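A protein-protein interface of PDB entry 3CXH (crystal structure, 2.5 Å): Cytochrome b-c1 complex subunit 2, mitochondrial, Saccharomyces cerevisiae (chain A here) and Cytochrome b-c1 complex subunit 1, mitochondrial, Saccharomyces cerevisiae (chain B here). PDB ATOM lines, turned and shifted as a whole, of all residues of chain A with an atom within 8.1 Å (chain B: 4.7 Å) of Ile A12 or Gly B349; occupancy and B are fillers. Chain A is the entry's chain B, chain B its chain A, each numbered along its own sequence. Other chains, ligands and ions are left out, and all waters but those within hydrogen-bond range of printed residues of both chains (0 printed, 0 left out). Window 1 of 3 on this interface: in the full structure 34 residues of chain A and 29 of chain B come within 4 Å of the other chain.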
ATOM      1  N   ARG A   6      10.501  38.444  17.501  1.00  0.00           N
ATOM      2  CA  ARG A   6       9.298  38.609  16.690  1.00  0.00           C
ATOM      3  C   ARG A   6       8.460  37.335  16.835  1.00  0.00           C
ATOM      4  O   ARG A   6       8.878  36.263  16.401  1.00  0.00           O
ATOM      5  CB  ARG A   6       9.669  38.849  15.221  1.00  0.00           C
ATOM      6  CG  ARG A   6       8.480  38.825  14.263  1.00  0.00           C
ATOM      7  CD  ARG A   6       8.833  39.376  12.879  1.00  0.00           C
ATOM      8  NE  ARG A   6       9.865  38.602  12.188  1.00  0.00           N
ATOM      9  CZ  ARG A   6      10.467  38.988  11.063  1.00  0.00           C
ATOM     10  NH1 ARG A   6      11.394  38.221  10.503  1.00  0.00           N
ATOM     11  NH2 ARG A   6      10.147  40.144  10.495  1.00  0.00           N
ATOM     12  N   ASP A   7       7.284  37.459  17.449  1.00  0.00           N
ATOM     13  CA  ASP A   7       6.394  36.321  17.678  1.00  0.00           C
ATOM     14  C   ASP A   7       5.485  35.961  16.497  1.00  0.00           C
ATOM     15  O   ASP A   7       5.377  36.711  15.523  1.00  0.00           O
ATOM     16  CB  ASP A   7       5.545  36.569  18.931  1.00  0.00           C
ATOM     17  CG  ASP A   7       5.019  35.282  19.557  1.00  0.00           C
ATOM     18  OD1 ASP A   7       3.917  35.304  20.148  1.00  0.00           O
ATOM     19  OD2 ASP A   7       5.716  34.249  19.471  1.00  0.00           O
ATOM     20  N   ALA A   8       4.868  34.781  16.596  1.00  0.00           N
ATOM     21  CA  ALA A   8       3.947  34.225  15.598  1.00  0.00           C
ATOM     22  C   ALA A   8       3.337  32.953  16.203  1.00  0.00           C
ATOM     23  O   ALA A   8       3.940  32.334  17.077  1.00  0.00           O
ATOM     24  CB  ALA A   8       4.685  33.899  14.301  1.00  0.00           C
ATOM     25  N   PRO A   9       2.135  32.550  15.751  1.00  0.00           N
ATOM     26  CA  PRO A   9       1.458  31.351  16.268  1.00  0.00           C
ATOM     27  C   PRO A   9       1.923  30.025  15.648  1.00  0.00           C
ATOM     28  O   PRO A   9       1.113  29.131  15.376  1.00  0.00           O
ATOM     29  CB  PRO A   9      -0.002  31.638  15.941  1.00  0.00           C
ATOM     30  CG  PRO A   9       0.117  32.287  14.592  1.00  0.00           C
ATOM     31  CD  PRO A   9       1.276  33.253  14.778  1.00  0.00           C
ATOM     32  N   THR A  10       3.233  29.899  15.453  1.00  0.00           N
ATOM     33  CA  THR A  10       3.826  28.698  14.873  1.00  0.00           C
ATOM     34  C   THR A  10       4.123  27.610  15.909  1.00  0.00           C
ATOM     35  O   THR A  10       3.946  27.809  17.117  1.00  0.00           O
ATOM     36  CB  THR A  10       5.140  29.030  14.149  1.00  0.00           C
ATOM     37  OG1 THR A  10       6.044  29.653  15.071  1.00  0.00           O
ATOM     38  CG2 THR A  10       4.884  29.958  12.974  1.00  0.00           C
ATOM     39  N   LYS A  11       4.580  26.462  15.416  1.00  0.00           N
ATOM     40  CA  LYS A  11       4.929  25.322  16.258  1.00  0.00           C
ATOM     41  C   LYS A  11       6.419  25.316  16.595  1.00  0.00           C
ATOM     42  O   LYS A  11       6.823  24.811  17.641  1.00  0.00           O
ATOM     43  CB  LYS A  11       4.548  24.015  15.560  1.00  0.00           C
ATOM     44  CG  LYS A  11       3.066  23.685  15.605  1.00  0.00           C
ATOM     45  CD  LYS A  11       2.641  23.359  17.029  1.00  0.00           C
ATOM     46  CE  LYS A  11       1.227  22.783  17.108  1.00  0.00           C
ATOM     47  NZ  LYS A  11       0.157  23.808  16.967  1.00  0.00           N
ATOM     48  N   ILE A  12       7.212  25.933  15.727  1.00  0.00           N
ATOM     49  CA  ILE A  12       8.660  26.000  15.878  1.00  0.00           C
ATOM     50  C   ILE A  12       9.154  27.419  16.126  1.00  0.00           C
ATOM     51  O   ILE A  12       8.557  28.381  15.652  1.00  0.00           O
ATOM     52  CB  ILE A  12       9.356  25.430  14.601  1.00  0.00           C
ATOM     53  CG1 ILE A  12       9.113  23.927  14.505  1.00  0.00           C
ATOM     54  CG2 ILE A  12      10.853  25.709  14.593  1.00  0.00           C
ATOM     55  CD1 ILE A  12       9.550  23.161  15.736  1.00  0.00           C
ATOM     56  N   SER A  13      10.256  27.530  16.866  1.00  0.00           N
ATOM     57  CA  SER A  13      10.894  28.809  17.185  1.00  0.00           C
ATOM     58  C   SER A  13      12.383  28.667  16.901  1.00  0.00           C
ATOM     59  O   SER A  13      12.866  27.567  16.636  1.00  0.00           O
ATOM     60  CB  SER A  13      10.710  29.154  18.664  1.00  0.00           C
ATOM     61  OG  SER A  13       9.338  29.206  19.016  1.00  0.00           O
ATOM     62  N   THR A  14      13.116  29.771  16.972  1.00  0.00           N
ATOM     63  CA  THR A  14      14.552  29.722  16.727  1.00  0.00           C
ATOM     64  C   THR A  14      15.353  30.799  17.461  1.00  0.00           C
ATOM     65  O   THR A  14      15.360  31.968  17.078  1.00  0.00           O
ATOM     66  CB  THR A  14      14.887  29.693  15.197  1.00  0.00           C
ATOM     67  OG1 THR A  14      16.264  30.033  14.996  1.00  0.00           O
ATOM     68  CG2 THR A  14      14.005  30.646  14.409  1.00  0.00           C
ATOM     69  N   LEU A  15      16.029  30.373  18.525  1.00  0.00           N
ATOM     70  CA  LEU A  15      16.855  31.240  19.364  1.00  0.00           C
ATOM     71  C   LEU A  15      18.217  31.453  18.712  1.00  0.00           C
ATOM     72  O   LEU A  15      18.758  30.547  18.091  1.00  0.00           O
ATOM     73  CB  LEU A  15      17.063  30.571  20.724  1.00  0.00           C
ATOM     74  CG  LEU A  15      17.142  31.367  22.027  1.00  0.00           C
ATOM     75  CD1 LEU A  15      18.107  32.527  21.909  1.00  0.00           C
ATOM     76  CD2 LEU A  15      15.765  31.866  22.387  1.00  0.00           C
ATOM     77  N   LEU A  58      13.340  16.277  23.355  1.00  0.00           N
ATOM     78  CA  LEU A  58      12.513  17.472  23.439  1.00  0.00           C
ATOM     79  C   LEU A  58      12.008  17.843  22.059  1.00  0.00           C
ATOM     80  O   LEU A  58      10.841  18.195  21.884  1.00  0.00           O
ATOM     81  CB  LEU A  58      13.310  18.649  24.003  1.00  0.00           C
ATOM     82  CG  LEU A  58      13.632  18.657  25.492  1.00  0.00           C
ATOM     83  CD1 LEU A  58      14.303  19.966  25.843  1.00  0.00           C
ATOM     84  CD2 LEU A  58      12.371  18.486  26.298  1.00  0.00           C
ATOM     85  N   GLY A  59      12.915  17.776  21.088  1.00  0.00           N
ATOM     86  CA  GLY A  59      12.584  18.121  19.723  1.00  0.00           C
ATOM     87  C   GLY A  59      13.296  19.396  19.316  1.00  0.00           C
ATOM     88  O   GLY A  59      12.659  20.361  18.908  1.00  0.00           O
ATOM     89  N   GLY A  60      14.618  19.407  19.442  1.00  0.00           N
ATOM     90  CA  GLY A  60      15.394  20.572  19.062  1.00  0.00           C
ATOM     91  C   GLY A  60      16.826  20.211  18.707  1.00  0.00           C
ATOM     92  O   GLY A  60      17.314  19.148  19.103  1.00  0.00           O
ATOM     93  N   ALA A  75      19.569  27.873  17.918  1.00  0.00           N
ATOM     94  CA  ALA A  75      18.750  26.737  18.321  1.00  0.00           C
ATOM     95  C   ALA A  75      17.382  26.766  17.654  1.00  0.00           C
ATOM     96  O   ALA A  75      16.749  27.812  17.570  1.00  0.00           O
ATOM     97  CB  ALA A  75      18.583  26.733  19.826  1.00  0.00           C
ATOM     98  N   THR A  76      16.936  25.607  17.181  1.00  0.00           N
ATOM     99  CA  THR A  76      15.637  25.460  16.533  1.00  0.00           C
ATOM    100  C   THR A  76      14.940  24.413  17.389  1.00  0.00           C
ATOM    101  O   THR A  76      15.501  23.338  17.620  1.00  0.00           O
ATOM    102  CB  THR A  76      15.789  24.931  15.101  1.00  0.00           C
ATOM    103  OG1 THR A  76      16.795  25.686  14.417  1.00  0.00           O
ATOM    104  CG2 THR A  76      14.483  25.062  14.353  1.00  0.00           C
ATOM    105  N   PHE A  77      13.716  24.698  17.830  1.00  0.00           N
ATOM    106  CA  PHE A  77      13.011  23.788  18.728  1.00  0.00           C
ATOM    107  C   PHE A  77      11.510  24.039  18.788  1.00  0.00           C
ATOM    108  O   PHE A  77      11.014  25.010  18.222  1.00  0.00           O
ATOM    109  CB  PHE A  77      13.569  24.008  20.125  1.00  0.00           C
ATOM    110  CG  PHE A  77      13.584  25.453  20.523  1.00  0.00           C
ATOM    111  CD1 PHE A  77      12.490  26.026  21.176  1.00  0.00           C
ATOM    112  CD2 PHE A  77      14.655  26.271  20.174  1.00  0.00           C
ATOM    113  CE1 PHE A  77      12.463  27.391  21.466  1.00  0.00           C
ATOM    114  CE2 PHE A  77      14.636  27.641  20.461  1.00  0.00           C
ATOM    115  CZ  PHE A  77      13.538  28.199  21.106  1.00  0.00           C
ATOM    116  N   LEU A  78      10.799  23.176  19.514  1.00  0.00           N
ATOM    117  CA  LEU A  78       9.356  23.315  19.695  1.00  0.00           C
ATOM    118  C   LEU A  78       9.137  24.478  20.661  1.00  0.00           C
ATOM    119  O   LEU A  78       9.586  24.430  21.810  1.00  0.00           O
ATOM    120  CB  LEU A  78       8.749  22.032  20.267  1.00  0.00           C
ATOM    121  CG  LEU A  78       8.893  20.755  19.433  1.00  0.00           C
ATOM    122  CD1 LEU A  78       8.309  19.590  20.199  1.00  0.00           C
ATOM    123  CD2 LEU A  78       8.202  20.906  18.092  1.00  0.00           C
ATOM    124  N   LYS A  79       8.447  25.510  20.168  1.00  0.00           N
ATOM    125  CA  LYS A  79       8.155  26.761  20.882  1.00  0.00           C
ATOM    126  C   LYS A  79       8.066  26.776  22.411  1.00  0.00           C
ATOM    127  O   LYS A  79       8.760  27.561  23.059  1.00  0.00           O
ATOM    128  CB  LYS A  79       6.910  27.423  20.280  1.00  0.00           C
ATOM    129  CG  LYS A  79       6.600  28.813  20.830  1.00  0.00           C
ATOM    130  CD  LYS A  79       5.545  29.517  19.990  1.00  0.00           C
ATOM    131  CE  LYS A  79       5.085  30.805  20.646  1.00  0.00           C
ATOM    132  NZ  LYS A  79       6.206  31.759  20.851  1.00  0.00           N
ATOM    133  N   ASP A  80       7.236  25.905  22.976  1.00  0.00           N
ATOM    134  CA  ASP A  80       7.039  25.847  24.425  1.00  0.00           C
ATOM    135  C   ASP A  80       8.225  25.438  25.305  1.00  0.00           C
ATOM    136  O   ASP A  80       8.126  25.499  26.528  1.00  0.00           O
ATOM    137  CB  ASP A  80       5.829  24.964  24.752  1.00  0.00           C
ATOM    138  CG  ASP A  80       4.498  25.644  24.443  1.00  0.00           C
ATOM    139  OD1 ASP A  80       4.468  26.620  23.656  1.00  0.00           O
ATOM    140  OD2 ASP A  80       3.473  25.201  25.002  1.00  0.00           O
ATOM    141  N   GLU A 174      12.916  34.249  17.192  1.00  0.00           N
ATOM    142  CA  GLU A 174      12.029  34.212  16.037  1.00  0.00           C
ATOM    143  C   GLU A 174      10.925  33.214  16.366  1.00  0.00           C
ATOM    144  O   GLU A 174      11.201  32.049  16.669  1.00  0.00           O
ATOM    145  CB  GLU A 174      12.806  33.784  14.794  1.00  0.00           C
ATOM    146  CG  GLU A 174      12.127  34.120  13.480  1.00  0.00           C
ATOM    147  CD  GLU A 174      11.878  35.612  13.310  1.00  0.00           C
ATOM    148  OE1 GLU A 174      12.857  36.396  13.335  1.00  0.00           O
ATOM    149  OE2 GLU A 174      10.694  35.994  13.155  1.00  0.00           O
ATOM    150  N   ASN A 175       9.680  33.688  16.305  1.00  0.00           N
ATOM    151  CA  ASN A 175       8.488  32.906  16.655  1.00  0.00           C
ATOM    152  C   ASN A 175       8.537  32.706  18.173  1.00  0.00           C
ATOM    153  O   ASN A 175       8.067  31.702  18.708  1.00  0.00           O
ATOM    154  CB  ASN A 175       8.450  31.566  15.914  1.00  0.00           C
ATOM    155  CG  ASN A 175       8.229  31.729  14.416  1.00  0.00           C
ATOM    156  OD1 ASN A 175       8.128  32.844  13.907  1.00  0.00           O
ATOM    157  ND2 ASN A 175       8.145  30.610  13.705  1.00  0.00           N
ATOM    158  N   VAL A 176       9.087  33.716  18.846  1.00  0.00           N
ATOM    159  CA  VAL A 176       9.274  33.745  20.296  1.00  0.00           C
ATOM    160  C   VAL A 176       8.639  34.995  20.919  1.00  0.00           C
ATOM    161  O   VAL A 176       8.719  36.087  20.351  1.00  0.00           O
ATOM    162  CB  VAL A 176      10.788  33.774  20.628  1.00  0.00           C
ATOM    163  CG1 VAL A 176      11.012  33.859  22.129  1.00  0.00           C
ATOM    164  CG2 VAL A 176      11.484  32.559  20.032  1.00  0.00           C
ATOM    165  N   LYS B 345       8.385  15.929  14.431  1.00  0.00           N
ATOM    166  CA  LYS B 345       7.672  17.195  14.579  1.00  0.00           C
ATOM    167  C   LYS B 345       8.575  18.347  14.185  1.00  0.00           C
ATOM    168  O   LYS B 345       8.201  19.199  13.372  1.00  0.00           O
ATOM    169  CB  LYS B 345       7.236  17.402  16.017  1.00  0.00           C
ATOM    170  CG  LYS B 345       6.149  16.487  16.503  1.00  0.00           C
ATOM    171  CD  LYS B 345       5.828  16.859  17.929  1.00  0.00           C
ATOM    172  CE  LYS B 345       4.856  15.889  18.543  1.00  0.00           C
ATOM    173  NZ  LYS B 345       4.454  16.339  19.908  1.00  0.00           N
ATOM    174  N   LEU B 346       9.770  18.369  14.767  1.00  0.00           N
ATOM    175  CA  LEU B 346      10.749  19.404  14.477  1.00  0.00           C
ATOM    176  C   LEU B 346      11.022  19.527  12.976  1.00  0.00           C
ATOM    177  O   LEU B 346      11.075  20.640  12.449  1.00  0.00           O
ATOM    178  CB  LEU B 346      12.060  19.115  15.216  1.00  0.00           C
ATOM    179  CG  LEU B 346      13.248  20.052  14.954  1.00  0.00           C
ATOM    180  CD1 LEU B 346      12.973  21.420  15.581  1.00  0.00           C
ATOM    181  CD2 LEU B 346      14.533  19.452  15.517  1.00  0.00           C
ATOM    182  N   GLN B 347      11.174  18.391  12.289  1.00  0.00           N
ATOM    183  CA  GLN B 347      11.453  18.421  10.855  1.00  0.00           C
ATOM    184  C   GLN B 347      10.266  18.930  10.038  1.00  0.00           C
ATOM    185  O   GLN B 347      10.446  19.762   9.149  1.00  0.00           O
ATOM    186  CB  GLN B 347      11.947  17.063  10.326  1.00  0.00           C
ATOM    187  CG  GLN B 347      10.872  16.028  10.040  1.00  0.00           C
ATOM    188  CD  GLN B 347      11.212  15.142   8.849  1.00  0.00           C
ATOM    189  OE1 GLN B 347      11.699  15.620   7.826  1.00  0.00           O
ATOM    190  NE2 GLN B 347      10.941  13.849   8.974  1.00  0.00           N
ATOM    191  N   LEU B 348       9.060  18.445  10.350  1.00  0.00           N
ATOM    192  CA  LEU B 348       7.861  18.884   9.646  1.00  0.00           C
ATOM    193  C   LEU B 348       7.683  20.382   9.878  1.00  0.00           C
ATOM    194  O   LEU B 348       7.234  21.114   8.993  1.00  0.00           O
ATOM    195  CB  LEU B 348       6.633  18.105  10.119  1.00  0.00           C
ATOM    196  CG  LEU B 348       6.586  16.633   9.680  1.00  0.00           C
ATOM    197  CD1 LEU B 348       5.295  15.985  10.151  1.00  0.00           C
ATOM    198  CD2 LEU B 348       6.715  16.518   8.161  1.00  0.00           C
ATOM    199  N   GLY B 349       8.082  20.833  11.063  1.00  0.00           N
ATOM    200  CA  GLY B 349       7.999  22.242  11.379  1.00  0.00           C
ATOM    201  C   GLY B 349       8.931  23.020  10.468  1.00  0.00           C
ATOM    202  O   GLY B 349       8.502  23.940   9.782  1.00  0.00           O
ATOM    203  N   GLN B 350      10.196  22.612  10.410  1.00  0.00           N
ATOM    204  CA  GLN B 350      11.186  23.291   9.573  1.00  0.00           C
ATOM    205  C   GLN B 350      10.851  23.289   8.082  1.00  0.00           C
ATOM    206  O   GLN B 350      11.417  24.065   7.310  1.00  0.00           O
ATOM    207  CB  GLN B 350      12.564  22.658   9.768  1.00  0.00           C
ATOM    208  CG  GLN B 350      13.196  22.938  11.108  1.00  0.00           C
ATOM    209  CD  GLN B 350      14.507  22.208  11.282  1.00  0.00           C
ATOM    210  OE1 GLN B 350      14.528  21.008  11.558  1.00  0.00           O
ATOM    211  NE2 GLN B 350      15.610  22.923  11.113  1.00  0.00           N
ATOM    212  N   LEU B 351       9.950  22.398   7.683  1.00  0.00           N
ATOM    213  CA  LEU B 351       9.555  22.271   6.290  1.00  0.00           C
ATOM    214  C   LEU B 351       8.408  23.226   5.992  1.00  0.00           C
ATOM    215  O   LEU B 351       8.513  24.086   5.117  1.00  0.00           O
ATOM    216  CB  LEU B 351       9.109  20.828   6.008  1.00  0.00           C
ATOM    217  CG  LEU B 351       9.256  20.147   4.634  1.00  0.00           C
ATOM    218  CD1 LEU B 351       7.948  19.442   4.287  1.00  0.00           C
ATOM    219  CD2 LEU B 351       9.663  21.116   3.532  1.00  0.00           C
ATOM    220  N   TYR B 352       7.324  23.068   6.742  1.00  0.00           N
ATOM    221  CA  TYR B 352       6.123  23.872   6.574  1.00  0.00           C
ATOM    222  C   TYR B 352       6.197  25.276   7.165  1.00  0.00           C
ATOM    223  O   TYR B 352       5.576  26.200   6.638  1.00  0.00           O
ATOM    224  CB  TYR B 352       4.913  23.118   7.135  1.00  0.00           C
ATOM    225  CG  TYR B 352       4.587  21.856   6.369  1.00  0.00           C
ATOM    226  CD1 TYR B 352       4.006  21.922   5.106  1.00  0.00           C
ATOM    227  CD2 TYR B 352       4.881  20.601   6.895  1.00  0.00           C
ATOM    228  CE1 TYR B 352       3.725  20.771   4.382  1.00  0.00           C
ATOM    229  CE2 TYR B 352       4.605  19.441   6.182  1.00  0.00           C
ATOM    230  CZ  TYR B 352       4.025  19.532   4.924  1.00  0.00           C
ATOM    231  OH  TYR B 352       3.722  18.389   4.218  1.00  0.00           O
ATOM    232  N   GLU B 353       6.946  25.431   8.254  1.00  0.00           N
ATOM    233  CA  GLU B 353       7.091  26.729   8.898  1.00  0.00           C
ATOM    234  C   GLU B 353       8.390  27.398   8.527  1.00  0.00           C
ATOM    235  O   GLU B 353       9.082  27.972   9.369  1.00  0.00           O
ATOM    236  CB  GLU B 353       6.959  26.616  10.410  1.00  0.00           C
ATOM    237  CG  GLU B 353       5.611  26.077  10.821  1.00  0.00           C
ATOM    238  CD  GLU B 353       5.404  26.065  12.308  1.00  0.00           C
ATOM    239  OE1 GLU B 353       6.403  26.087  13.057  1.00  0.00           O
ATOM    240  OE2 GLU B 353       4.232  26.029  12.730  1.00  0.00           O
ATOM    241  N   SER B 354       8.732  27.283   7.253  1.00  0.00           N
ATOM    242  CA  SER B 354       9.922  27.912   6.712  1.00  0.00           C
ATOM    243  C   SER B 354       9.573  29.391   6.526  1.00  0.00           C
ATOM    244  O   SER B 354       8.404  29.746   6.317  1.00  0.00           O
ATOM    245  CB  SER B 354      10.253  27.289   5.359  1.00  0.00           C
ATOM    246  OG  SER B 354      11.262  28.024   4.700  1.00  0.00           O
ATOM    247  N   LEU B 377      -0.491  21.628  10.362  1.00  0.00           N
ATOM    248  CA  LEU B 377       0.583  21.136  11.212  1.00  0.00           C
ATOM    249  C   LEU B 377       0.093  20.615  12.562  1.00  0.00           C
ATOM    250  O   LEU B 377       0.615  19.631  13.078  1.00  0.00           O
ATOM    251  CB  LEU B 377       1.632  22.233  11.394  1.00  0.00           C
ATOM    252  CG  LEU B 377       3.035  21.773  11.772  1.00  0.00           C
ATOM    253  CD1 LEU B 377       3.498  20.670  10.837  1.00  0.00           C
ATOM    254  CD2 LEU B 377       3.975  22.947  11.697  1.00  0.00           C
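N of Ser A13 lies within hydrogen-bond range of O of Phe A77. OG1 of Thr A10 is in hydrogen-bond range of ND2 of Asn A175 (2.7 Å). The backbone carbonyl oxygen of Lys A11 sits at hydrogen-bond distance from the backbone NH of Lys A79, 3.1 Å away. The backbone carbonyl oxygen (O) of Gly A59 lies within hydrogen-bond range of the backbone NH (N) of Leu A78. The side-chain hydroxyl of Thr A10 sits at hydrogen-bond distance from the backbone carbonyl oxygen of Ile A12 (2.9 Å). The backbone carbonyl oxygen (O) of Ile A12 lies within hydrogen-bond range of the side-chain amide nitrogen (ND2) of Asn A175 (3.0 Å).
Gly B349 touches just one residue of chain A: Ile A12 (3.7 Å). Of the printed residues of chain B, Thr A76 touches Leu B346 (3.8 Å). Printed residues of chain B within 4 Å of Thr A10: Glu B353 (3.4 Å). Of the printed residues of chain A, Glu B353 touches Thr A10 (3.4 Å), Lys A11 (2.7 Å) and Ile A12 (2.8 Å). The nearest residue of chain B that does not touch Ile A12 is Gln B350 (4.4 Å). The nearest printed residue of chain B that does not touch Lys A11 is Leu B377 (4.05 Å).
Among the printed residues, merely in contact across the chains: Thr A10 with Glu B353 (3.4 Å), Gly A59 with Leu B346 (3.5 Å), Ile A12 with Gly B349 (3.7 Å), Thr A76 with Leu B346 (3.8 Å), Gly A60 with Leu B346 (3.8 Å), Ile A12 with Leu B346 (3.8 Å) and Phe A77 with Leu B346 (3.9 Å).
Along chain A the printed residues that touch a printed residue of chain B span positions 10 to 77. Along chain B the printed residues that touch a printed residue of chain A span positions 346 to 353. Among the printed residues, no Asp or Glu carboxylate lies within 4 Å of a Lys or Arg side-chain nitrogen of the other chain.
N of Ile A12 sits at hydrogen-bond distance from OE1 of Glu B353 (2.8 Å). OE2 of Glu B353 sits at hydrogen-bond distance from N of Lys A11 (2.7 Å).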
